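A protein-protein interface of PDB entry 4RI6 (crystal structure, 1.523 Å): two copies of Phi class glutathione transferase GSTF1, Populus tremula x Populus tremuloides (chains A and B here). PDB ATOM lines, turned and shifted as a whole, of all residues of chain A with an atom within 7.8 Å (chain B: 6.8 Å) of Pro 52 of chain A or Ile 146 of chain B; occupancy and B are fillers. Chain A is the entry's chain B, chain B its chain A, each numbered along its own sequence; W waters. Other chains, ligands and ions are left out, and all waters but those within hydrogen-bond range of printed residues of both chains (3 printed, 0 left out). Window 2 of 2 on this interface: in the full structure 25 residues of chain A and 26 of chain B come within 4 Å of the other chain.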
ATOM      1  N   GLN A  42       3.694  20.799  20.807  1.00  0.00           N
ATOM      2  CA  GLN A  42       2.822  19.749  21.299  1.00  0.00           C
ATOM      3  C   GLN A  42       3.250  18.343  20.842  1.00  0.00           C
ATOM      4  O   GLN A  42       2.770  17.349  21.388  1.00  0.00           O
ATOM      5  CB  GLN A  42       1.392  20.032  20.851  1.00  0.00           C
ATOM      6  CG  GLN A  42       1.074  19.692  19.376  1.00  0.00           C
ATOM      7  CD  GLN A  42       1.544  20.734  18.356  1.00  0.00           C
ATOM      8  OE1 GLN A  42       2.395  21.588  18.625  1.00  0.00           O
ATOM      9  NE2 GLN A  42       0.983  20.644  17.163  1.00  0.00           N
ATOM     10  N   LYS A  43       4.134  18.277  19.843  1.00  0.00           N
ATOM     11  CA  LYS A  43       4.524  17.009  19.218  1.00  0.00           C
ATOM     12  C   LYS A  43       5.883  16.538  19.662  1.00  0.00           C
ATOM     13  O   LYS A  43       6.363  15.495  19.199  1.00  0.00           O
ATOM     14  CB  LYS A  43       4.529  17.120  17.692  1.00  0.00           C
ATOM     15  CG  LYS A  43       3.187  17.461  17.091  1.00  0.00           C
ATOM     16  CD  LYS A  43       2.149  16.456  17.565  1.00  0.00           C
ATOM     17  CE  LYS A  43       1.033  16.297  16.560  1.00  0.00           C
ATOM     18  NZ  LYS A  43      -0.239  15.873  17.200  1.00  0.00           N
ATOM     19  N   TYR A  47       6.064  17.525  26.040  1.00  0.00           N
ATOM     20  CA  TYR A  47       4.639  17.660  26.160  1.00  0.00           C
ATOM     21  C   TYR A  47       3.951  16.279  26.023  1.00  0.00           C
ATOM     22  O   TYR A  47       2.913  16.040  26.634  1.00  0.00           O
ATOM     23  CB  TYR A  47       4.119  18.660  25.143  1.00  0.00           C
ATOM     24  CG  TYR A  47       2.660  18.837  25.315  1.00  0.00           C
ATOM     25  CD1 TYR A  47       2.152  19.499  26.426  1.00  0.00           C
ATOM     26  CD2 TYR A  47       1.777  18.297  24.401  1.00  0.00           C
ATOM     27  CE1 TYR A  47       0.804  19.618  26.607  1.00  0.00           C
ATOM     28  CE2 TYR A  47       0.421  18.429  24.564  1.00  0.00           C
ATOM     29  CZ  TYR A  47      -0.065  19.090  25.672  1.00  0.00           C
ATOM     30  OH  TYR A  47      -1.419  19.223  25.852  1.00  0.00           O
ATOM     31  N   LEU A  48       4.555  15.347  25.291  1.00  0.00           N
ATOM     32  CA  LEU A  48       3.915  14.034  25.107  1.00  0.00           C
ATOM     33  C   LEU A  48       3.759  13.232  26.404  1.00  0.00           C
ATOM     34  O   LEU A  48       2.918  12.368  26.495  1.00  0.00           O
ATOM     35  CB  LEU A  48       4.678  13.194  24.077  1.00  0.00           C
ATOM     36  CG  LEU A  48       4.538  13.681  22.633  1.00  0.00           C
ATOM     37  CD1 LEU A  48       5.355  12.813  21.699  1.00  0.00           C
ATOM     38  CD2 LEU A  48       3.072  13.732  22.169  1.00  0.00           C
ATOM     39  N   LYS A  49       4.582  13.510  27.400  1.00  0.00           N
ATOM     40  CA  LYS A  49       4.420  12.858  28.691  1.00  0.00           C
ATOM     41  C   LYS A  49       3.091  13.221  29.355  1.00  0.00           C
ATOM     42  O   LYS A  49       2.570  12.461  30.169  1.00  0.00           O
ATOM     43  CB  LYS A  49       5.570  13.234  29.625  1.00  0.00           C
ATOM     44  CG  LYS A  49       6.923  12.677  29.209  1.00  0.00           C
ATOM     45  CD  LYS A  49       7.985  13.150  30.187  1.00  0.00           C
ATOM     46  CE  LYS A  49       9.368  12.620  29.858  1.00  0.00           C
ATOM     47  NZ  LYS A  49      10.361  13.110  30.859  1.00  0.00           N
ATOM     48  N   ILE A  50       2.546  14.380  28.998  1.00  0.00           N
ATOM     49  CA  ILE A  50       1.344  14.894  29.644  1.00  0.00           C
ATOM     50  C   ILE A  50       0.117  14.596  28.812  1.00  0.00           C
ATOM     51  O   ILE A  50      -0.943  14.282  29.345  1.00  0.00           O
ATOM     52  CB  ILE A  50       1.454  16.418  29.889  1.00  0.00           C
ATOM     53  CG1 ILE A  50       2.662  16.714  30.791  1.00  0.00           C
ATOM     54  CG2 ILE A  50       0.188  16.952  30.534  1.00  0.00           C
ATOM     55  CD1 ILE A  50       3.088  18.176  30.823  1.00  0.00           C
ATOM     56  N   GLN A  51       0.268  14.699  27.498  1.00  0.00           N
ATOM     57  CA  GLN A  51      -0.832  14.445  26.584  1.00  0.00           C
ATOM     58  C   GLN A  51      -0.270  13.543  25.501  1.00  0.00           C
ATOM     59  O   GLN A  51       0.463  13.993  24.607  1.00  0.00           O
ATOM     60  CB  GLN A  51      -1.406  15.763  26.033  1.00  0.00           C
ATOM     61  CG  GLN A  51      -2.928  15.735  25.870  1.00  0.00           C
ATOM     62  CD  GLN A  51      -3.379  14.938  24.663  1.00  0.00           C
ATOM     63  OE1 GLN A  51      -2.589  14.231  24.040  1.00  0.00           O
ATOM     64  NE2 GLN A  51      -4.658  15.038  24.335  1.00  0.00           N
ATOM     65  N   PRO A  52      -0.573  12.245  25.605  1.00  0.00           N
ATOM     66  CA  PRO A  52       0.215  11.295  24.805  1.00  0.00           C
ATOM     67  C   PRO A  52      -0.111  11.326  23.317  1.00  0.00           C
ATOM     68  O   PRO A  52       0.629  10.741  22.529  1.00  0.00           O
ATOM     69  CB  PRO A  52      -0.145   9.937  25.423  1.00  0.00           C
ATOM     70  CG  PRO A  52      -1.488  10.142  26.037  1.00  0.00           C
ATOM     71  CD  PRO A  52      -1.584  11.579  26.442  1.00  0.00           C
ATOM     72  N   PHE A  53      -1.190  12.013  22.944  1.00  0.00           N
ATOM     73  CA  PHE A  53      -1.574  12.148  21.544  1.00  0.00           C
ATOM     74  C   PHE A  53      -1.011  13.431  20.956  1.00  0.00           C
ATOM     75  O   PHE A  53      -1.205  13.713  19.779  1.00  0.00           O
ATOM     76  CB  PHE A  53      -3.104  12.093  21.402  1.00  0.00           C
ATOM     77  CG  PHE A  53      -3.667  10.786  21.851  1.00  0.00           C
ATOM     78  CD1 PHE A  53      -3.622   9.694  21.010  1.00  0.00           C
ATOM     79  CD2 PHE A  53      -4.166  10.621  23.131  1.00  0.00           C
ATOM     80  CE1 PHE A  53      -4.079   8.468  21.422  1.00  0.00           C
ATOM     81  CE2 PHE A  53      -4.639   9.379  23.542  1.00  0.00           C
ATOM     82  CZ  PHE A  53      -4.591   8.317  22.682  1.00  0.00           C
ATOM     83  N   GLY A  54      -0.301  14.196  21.771  1.00  0.00           N
ATOM     84  CA  GLY A  54       0.331  15.410  21.295  1.00  0.00           C
ATOM     85  C   GLY A  54      -0.703  16.452  20.918  1.00  0.00           C
ATOM     86  O   GLY A  54      -0.580  17.144  19.910  1.00  0.00           O
ATOM     87  N   GLN A  55      -1.750  16.536  21.725  1.00  0.00           N
ATOM     88  CA  GLN A  55      -2.794  17.507  21.496  1.00  0.00           C
ATOM     89  C   GLN A  55      -3.056  18.339  22.735  1.00  0.00           C
ATOM     90  O   GLN A  55      -2.674  17.977  23.826  1.00  0.00           O
ATOM     91  CB  GLN A  55      -4.064  16.798  21.040  1.00  0.00           C
ATOM     92  CG  GLN A  55      -3.855  16.108  19.715  1.00  0.00           C
ATOM     93  CD  GLN A  55      -5.066  15.348  19.234  1.00  0.00           C
ATOM     94  OE1 GLN A  55      -5.863  14.834  20.027  1.00  0.00           O
ATOM     95  NE2 GLN A  55      -5.209  15.262  17.916  1.00  0.00           N
ATOM     96  N   ALA A  58      -4.187  19.914  28.045  1.00  0.00           N
ATOM     97  CA  ALA A  58      -4.030  19.061  29.192  1.00  0.00           C
ATOM     98  C   ALA A  58      -4.365  19.842  30.434  1.00  0.00           C
ATOM     99  O   ALA A  58      -4.298  21.077  30.449  1.00  0.00           O
ATOM    100  CB  ALA A  58      -2.627  18.505  29.269  1.00  0.00           C
ATOM    101  N   LEU A  66      -5.142  15.177  33.579  1.00  0.00           N
ATOM    102  CA  LEU A  66      -6.176  14.693  32.670  1.00  0.00           C
ATOM    103  C   LEU A  66      -5.991  15.229  31.269  1.00  0.00           C
ATOM    104  O   LEU A  66      -5.481  16.335  31.080  1.00  0.00           O
ATOM    105  CB  LEU A  66      -7.563  15.085  33.175  1.00  0.00           C
ATOM    106  CG  LEU A  66      -8.074  14.413  34.447  1.00  0.00           C
ATOM    107  CD1 LEU A  66      -9.264  15.196  34.979  1.00  0.00           C
ATOM    108  CD2 LEU A  66      -8.452  12.964  34.177  1.00  0.00           C
ATOM    109  N   PHE A  67      -6.457  14.468  30.282  1.00  0.00           N
ATOM    110  CA  PHE A  67      -6.600  15.001  28.933  1.00  0.00           C
ATOM    111  C   PHE A  67      -8.007  14.693  28.412  1.00  0.00           C
ATOM    112  O   PHE A  67      -8.799  14.080  29.105  1.00  0.00           O
ATOM    113  CB  PHE A  67      -5.505  14.466  27.994  1.00  0.00           C
ATOM    114  CG  PHE A  67      -5.471  12.990  27.850  1.00  0.00           C
ATOM    115  CD1 PHE A  67      -6.164  12.358  26.844  1.00  0.00           C
ATOM    116  CD2 PHE A  67      -4.675  12.223  28.687  1.00  0.00           C
ATOM    117  CE1 PHE A  67      -6.096  10.995  26.697  1.00  0.00           C
ATOM    118  CE2 PHE A  67      -4.618  10.852  28.535  1.00  0.00           C
ATOM    119  CZ  PHE A  67      -5.340  10.254  27.550  1.00  0.00           C
ATOM    120  N   GLU A  68      -8.279  15.182  27.203  1.00  0.00           N
ATOM    121  CA  GLU A  68      -9.575  15.196  26.515  1.00  0.00           C
ATOM    122  C   GLU A  68     -10.509  16.231  27.146  1.00  0.00           C
ATOM    123  O   GLU A  68     -10.940  16.101  28.286  1.00  0.00           O
ATOM    124  CB  GLU A  68     -10.231  13.808  26.456  1.00  0.00           C
ATOM    125  CG  GLU A  68      -9.764  12.970  25.254  1.00  0.00           C
ATOM    126  CD  GLU A  68     -10.187  13.563  23.907  1.00  0.00           C
ATOM    127  OE1 GLU A  68     -11.031  14.461  23.903  1.00  0.00           O
ATOM    128  OE2 GLU A  68      -9.661  13.131  22.859  1.00  0.00           O
ATOM    129  N   TRP B 102     -10.105   8.200  28.956  1.00  0.00           N
ATOM    130  CA  TRP B 102      -9.883   7.125  27.977  1.00  0.00           C
ATOM    131  C   TRP B 102     -11.197   6.776  27.283  1.00  0.00           C
ATOM    132  O   TRP B 102     -11.193   6.331  26.141  1.00  0.00           O
ATOM    133  CB  TRP B 102      -9.235   5.900  28.646  1.00  0.00           C
ATOM    134  CG  TRP B 102      -7.845   6.216  29.065  1.00  0.00           C
ATOM    135  CD1 TRP B 102      -7.415   6.546  30.317  1.00  0.00           C
ATOM    136  CD2 TRP B 102      -6.697   6.297  28.216  1.00  0.00           C
ATOM    137  NE1 TRP B 102      -6.080   6.825  30.293  1.00  0.00           N
ATOM    138  CE2 TRP B 102      -5.616   6.687  29.016  1.00  0.00           C
ATOM    139  CE3 TRP B 102      -6.482   6.072  26.856  1.00  0.00           C
ATOM    140  CZ2 TRP B 102      -4.350   6.845  28.509  1.00  0.00           C
ATOM    141  CZ3 TRP B 102      -5.234   6.247  26.354  1.00  0.00           C
ATOM    142  CH2 TRP B 102      -4.178   6.615  27.171  1.00  0.00           C
ATOM    143  N   THR B 109     -10.959   9.697  19.266  1.00  0.00           N
ATOM    144  CA  THR B 109      -9.673   9.341  18.654  1.00  0.00           C
ATOM    145  C   THR B 109      -9.666   7.935  18.012  1.00  0.00           C
ATOM    146  O   THR B 109      -9.370   7.783  16.833  1.00  0.00           O
ATOM    147  CB  THR B 109      -8.566   9.489  19.726  1.00  0.00           C
ATOM    148  OG1 THR B 109      -8.592  10.845  20.188  1.00  0.00           O
ATOM    149  CG2 THR B 109      -7.190   9.144  19.157  1.00  0.00           C
ATOM    150  N   ALA B 141      -3.660   2.839  13.275  1.00  0.00           N
ATOM    151  CA  ALA B 141      -2.346   2.335  13.627  1.00  0.00           C
ATOM    152  C   ALA B 141      -1.613   3.313  14.532  1.00  0.00           C
ATOM    153  O   ALA B 141      -0.987   2.905  15.523  1.00  0.00           O
ATOM    154  CB  ALA B 141      -1.544   2.035  12.377  1.00  0.00           C
ATOM    155  N   LYS B 142      -1.705   4.603  14.215  1.00  0.00           N
ATOM    156  CA  LYS B 142      -1.088   5.632  15.052  1.00  0.00           C
ATOM    157  C   LYS B 142      -1.690   5.660  16.457  1.00  0.00           C
ATOM    158  O   LYS B 142      -0.966   5.795  17.439  1.00  0.00           O
ATOM    159  CB  LYS B 142      -1.211   7.015  14.388  1.00  0.00           C
ATOM    160  CG  LYS B 142      -0.316   7.170  13.142  1.00  0.00           C
ATOM    161  CD  LYS B 142       1.111   7.579  13.482  1.00  0.00           C
ATOM    162  CE  LYS B 142       2.115   6.983  12.493  1.00  0.00           C
ATOM    163  NZ  LYS B 142       3.548   7.089  12.921  1.00  0.00           N
ATOM    164  N   VAL B 143      -3.010   5.553  16.560  1.00  0.00           N
ATOM    165  CA  VAL B 143      -3.646   5.459  17.861  1.00  0.00           C
ATOM    166  C   VAL B 143      -3.140   4.239  18.634  1.00  0.00           C
ATOM    167  O   VAL B 143      -2.821   4.317  19.821  1.00  0.00           O
ATOM    168  CB  VAL B 143      -5.178   5.377  17.711  1.00  0.00           C
ATOM    169  CG1 VAL B 143      -5.847   5.181  19.031  1.00  0.00           C
ATOM    170  CG2 VAL B 143      -5.712   6.640  17.052  1.00  0.00           C
ATOM    171  N   LEU B 144      -3.102   3.096  17.966  1.00  0.00           N
ATOM    172  CA  LEU B 144      -2.716   1.855  18.648  1.00  0.00           C
ATOM    173  C   LEU B 144      -1.233   1.823  19.013  1.00  0.00           C
ATOM    174  O   LEU B 144      -0.859   1.129  19.967  1.00  0.00           O
ATOM    175  CB  LEU B 144      -3.097   0.652  17.793  1.00  0.00           C
ATOM    176  CG  LEU B 144      -4.620   0.469  17.646  1.00  0.00           C
ATOM    177  CD1 LEU B 144      -4.922  -0.690  16.703  1.00  0.00           C
ATOM    178  CD2 LEU B 144      -5.324   0.244  19.010  1.00  0.00           C
ATOM    179  N   ASP B 145      -0.392   2.605  18.325  1.00  0.00           N
ATOM    180  CA  ASP B 145       1.012   2.739  18.754  1.00  0.00           C
ATOM    181  C   ASP B 145       1.084   3.446  20.114  1.00  0.00           C
ATOM    182  O   ASP B 145       1.955   3.148  20.938  1.00  0.00           O
ATOM    183  CB  ASP B 145       1.851   3.506  17.727  1.00  0.00           C
ATOM    184  CG  ASP B 145       2.154   2.716  16.461  1.00  0.00           C
ATOM    185  OD1 ASP B 145       2.156   1.461  16.497  1.00  0.00           O
ATOM    186  OD2 ASP B 145       2.438   3.388  15.422  1.00  0.00           O
ATOM    187  N   ILE B 146       0.183   4.398  20.339  1.00  0.00           N
ATOM    188  CA  ILE B 146       0.106   5.080  21.617  1.00  0.00           C
ATOM    189  C   ILE B 146      -0.446   4.148  22.688  1.00  0.00           C
ATOM    190  O   ILE B 146       0.077   4.093  23.808  1.00  0.00           O
ATOM    191  CB  ILE B 146      -0.740   6.350  21.510  1.00  0.00           C
ATOM    192  CG1 ILE B 146      -0.054   7.310  20.550  1.00  0.00           C
ATOM    193  CG2 ILE B 146      -0.940   6.973  22.887  1.00  0.00           C
ATOM    194  CD1 ILE B 146      -0.881   8.447  20.122  1.00  0.00           C
ATOM    195  N   TYR B 147      -1.462   3.365  22.336  1.00  0.00           N
ATOM    196  CA  TYR B 147      -1.993   2.377  23.263  1.00  0.00           C
ATOM    197  C   TYR B 147      -0.938   1.343  23.610  1.00  0.00           C
ATOM    198  O   TYR B 147      -0.882   0.884  24.731  1.00  0.00           O
ATOM    199  CB  TYR B 147      -3.213   1.661  22.690  1.00  0.00           C
ATOM    200  CG  TYR B 147      -4.507   2.443  22.613  1.00  0.00           C
ATOM    201  CD1 TYR B 147      -4.545   3.826  22.758  1.00  0.00           C
ATOM    202  CD2 TYR B 147      -5.707   1.772  22.412  1.00  0.00           C
ATOM    203  CE1 TYR B 147      -5.756   4.506  22.674  1.00  0.00           C
ATOM    204  CE2 TYR B 147      -6.892   2.438  22.338  1.00  0.00           C
ATOM    205  CZ  TYR B 147      -6.913   3.802  22.471  1.00  0.00           C
ATOM    206  OH  TYR B 147      -8.123   4.441  22.392  1.00  0.00           O
ATOM    207  N   GLU B 148      -0.125   0.957  22.632  1.00  0.00           N
ATOM    208  CA  GLU B 148       0.916  -0.041  22.874  1.00  0.00           C
ATOM    209  C   GLU B 148       1.853   0.426  23.990  1.00  0.00           C
ATOM    210  O   GLU B 148       2.245  -0.348  24.845  1.00  0.00           O
ATOM    211  CB  GLU B 148       1.697  -0.319  21.594  1.00  0.00           C
ATOM    212  CG  GLU B 148       2.839  -1.339  21.761  1.00  0.00           C
ATOM    213  CD  GLU B 148       2.346  -2.739  22.093  1.00  0.00           C
ATOM    214  OE1 GLU B 148       1.125  -2.978  21.964  1.00  0.00           O
ATOM    215  OE2 GLU B 148       3.185  -3.594  22.477  1.00  0.00           O
ATOM    216  N   GLN B 149       2.189   1.714  23.978  1.00  0.00           N
ATOM    217  CA  GLN B 149       3.057   2.276  25.001  1.00  0.00           C
ATOM    218  C   GLN B 149       2.336   2.317  26.363  1.00  0.00           C
ATOM    219  O   GLN B 149       2.872   1.873  27.378  1.00  0.00           O
ATOM    220  CB  GLN B 149       3.553   3.672  24.556  1.00  0.00           C
ATOM    221  CG  GLN B 149       4.476   3.611  23.304  1.00  0.00           C
ATOM    222  CD  GLN B 149       4.701   4.948  22.561  1.00  0.00           C
ATOM    223  OE1 GLN B 149       3.761   5.683  22.244  1.00  0.00           O
ATOM    224  NE2 GLN B 149       5.965   5.233  22.241  1.00  0.00           N
ATOM    225  N   LYS B 150       1.105   2.809  26.367  1.00  0.00           N
ATOM    226  CA  LYS B 150       0.293   2.890  27.573  1.00  0.00           C
ATOM    227  C   LYS B 150       0.099   1.528  28.225  1.00  0.00           C
ATOM    228  O   LYS B 150       0.209   1.376  29.453  1.00  0.00           O
ATOM    229  CB  LYS B 150      -1.069   3.502  27.227  1.00  0.00           C
ATOM    230  CG  LYS B 150      -2.024   3.692  28.413  1.00  0.00           C
ATOM    231  CD  LYS B 150      -1.513   4.797  29.348  1.00  0.00           C
ATOM    232  CE  LYS B 150      -2.416   5.056  30.575  1.00  0.00           C
ATOM    233  NZ  LYS B 150      -2.388   3.953  31.551  1.00  0.00           N
ATOM    234  N   LEU B 151      -0.195   0.535  27.395  1.00  0.00           N
ATOM    235  CA  LEU B 151      -0.514  -0.804  27.891  1.00  0.00           C
ATOM    236  C   LEU B 151       0.755  -1.598  28.279  1.00  0.00           C
ATOM    237  O   LEU B 151       0.672  -2.697  28.809  1.00  0.00           O
ATOM    238  CB  LEU B 151      -1.363  -1.551  26.860  1.00  0.00           C
ATOM    239  CG  LEU B 151      -2.764  -0.936  26.717  1.00  0.00           C
ATOM    240  CD1 LEU B 151      -3.421  -1.411  25.464  1.00  0.00           C
ATOM    241  CD2 LEU B 151      -3.629  -1.234  27.921  1.00  0.00           C
ATOM    242  N   ARG B 189       0.709  -5.964  17.718  1.00  0.00           N
ATOM    243  CA  ARG B 189       1.204  -5.101  18.789  1.00  0.00           C
ATOM    244  C   ARG B 189       1.064  -5.879  20.097  1.00  0.00           C
ATOM    245  O   ARG B 189      -0.037  -6.177  20.528  1.00  0.00           O
ATOM    246  CB  ARG B 189       0.401  -3.795  18.817  1.00  0.00           C
ATOM    247  CG  ARG B 189       0.733  -2.868  17.664  1.00  0.00           C
ATOM    248  CD  ARG B 189      -0.220  -1.659  17.570  1.00  0.00           C
ATOM    249  NE  ARG B 189       0.289  -0.748  16.557  1.00  0.00           N
ATOM    250  CZ  ARG B 189       0.134  -0.905  15.248  1.00  0.00           C
ATOM    251  NH1 ARG B 189      -0.634  -1.869  14.759  1.00  0.00           N
ATOM    252  NH2 ARG B 189       0.765  -0.100  14.424  1.00  0.00           N
ATOM    253  N   VAL B 192      -1.073  -4.382  23.109  1.00  0.00           N
ATOM    254  CA  VAL B 192      -2.444  -4.224  22.621  1.00  0.00           C
ATOM    255  C   VAL B 192      -3.088  -5.590  22.460  1.00  0.00           C
ATOM    256  O   VAL B 192      -4.243  -5.781  22.804  1.00  0.00           O
ATOM    257  CB  VAL B 192      -2.467  -3.435  21.286  1.00  0.00           C
ATOM    258  CG1 VAL B 192      -3.840  -3.483  20.615  1.00  0.00           C
ATOM    259  CG2 VAL B 192      -2.089  -2.007  21.568  1.00  0.00           C
HETATM  260  O   HOH W   1      -8.903  13.487  19.232  1.00  0.00           O
HETATM  261  O   HOH W   2      -7.810  11.354  22.729  1.00  0.00           O
HETATM  262  O   HOH W   3      -6.231  12.505  19.357  1.00  0.00           O
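Of chain B, only Ile 146 comes within 4 Å of Pro 52 of chain A. Of the printed residues of chain A, Ile 146 of chain B touches Pro 52 (3.7 Å) and Phe 53 (3.1 Å). Of the printed residues of chain B, Phe 53 of chain A touches Thr 109 (3.9 Å), Ile 146 (3.1 Å) and Tyr 147 (3.99 Å). Of the printed residues of chain B, Glu 68 of chain A touches Thr 109. Printed residues of chain B within 4 Å of Phe 67 of chain A: Trp 102. Of the printed residues of chain A, Trp 102 of chain B touches Phe 67 (3.7 Å). Of the printed residues of chain A, Tyr 147 of chain B touches Phe 53. Val 192 of chain B touches none of the printed residues of chain A. Val 143 of chain B touches none of the printed residues of chain A. The nearest residue of chain B that does not touch Pro 52 of chain A is Trp 102 of chain B (4.6 Å). The nearest residue of chain A that does not touch Ile 146 of chain B is Gly 54 of chain A (6.0 Å). The nearest printed residue of chain B that does not touch Phe 53 of chain A is Trp 102 of chain B (4.3 Å).
Ile 146 of chain B touches Pro 52 of chain A. Thr 109 of chain B touches Phe 53 of chain A (CG2 to CE1, 3.9 Å). CD1 of Ile 146 of chain B touches CD1 of Phe 53 of chain A, 3.1 Å away. Tyr 147 of chain B touches Phe 53 of chain A (CE1 to CZ, 3.99 Å). CZ2 of Trp 102 of chain B touches CZ of Phe 67 of chain A (3.7 Å). OE2 of Glu 68 of chain A touches OG1 of Thr 109 of chain B, 3.7 Å away.
N of Phe 53 of chain A is in hydrogen-bond range of OE1 of Gln 51 of chain A, at 2.8 Å.
Of the 15 printed residues of chain A, 4 touch a printed residue of chain B. Printed residues of chain A that touch a printed residue of chain B: Pro 52, Phe 53, Phe 67 and Glu 68. Hydrophobic or aromatic side chains of chain A that line the printed part of chain B: Pro 52, Phe 53 and Phe 67. Of the 15 printed residues of chain B, 4 touch a printed residue of chain A. Hydrophobic or aromatic side chains of chain B that line the printed part of chain A: Trp 102, Ile 146 and Tyr 147. Along chain B the printed residues that touch a printed residue of chain A span positions 102 to 147. Among the printed residues, no Asp or Glu carboxylate lies within 4 Å of a Lys or Arg side-chain nitrogen of the other chain.
Water W3 bridges the side-chain amide oxygen of Gln 55 of chain A (2.5 Å) and the side-chain hydroxyl of Thr 109 of chain B (3.0 Å). Water W2 lies within hydrogen-bond range of OE2 of Glu 68 of chain A (2.6 Å) and OG1 of Thr 109 of chain B (2.7 Å). Water W1 bridges OG1 of Thr 109 of chain B (2.8 Å) and OE1 of Gln 55 of chain A (3.4 Å).
No position is printed for both chains. Of the 6 pairs that touch across the chains among the printed residues, none has its exchanged pair printed and touching as well.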
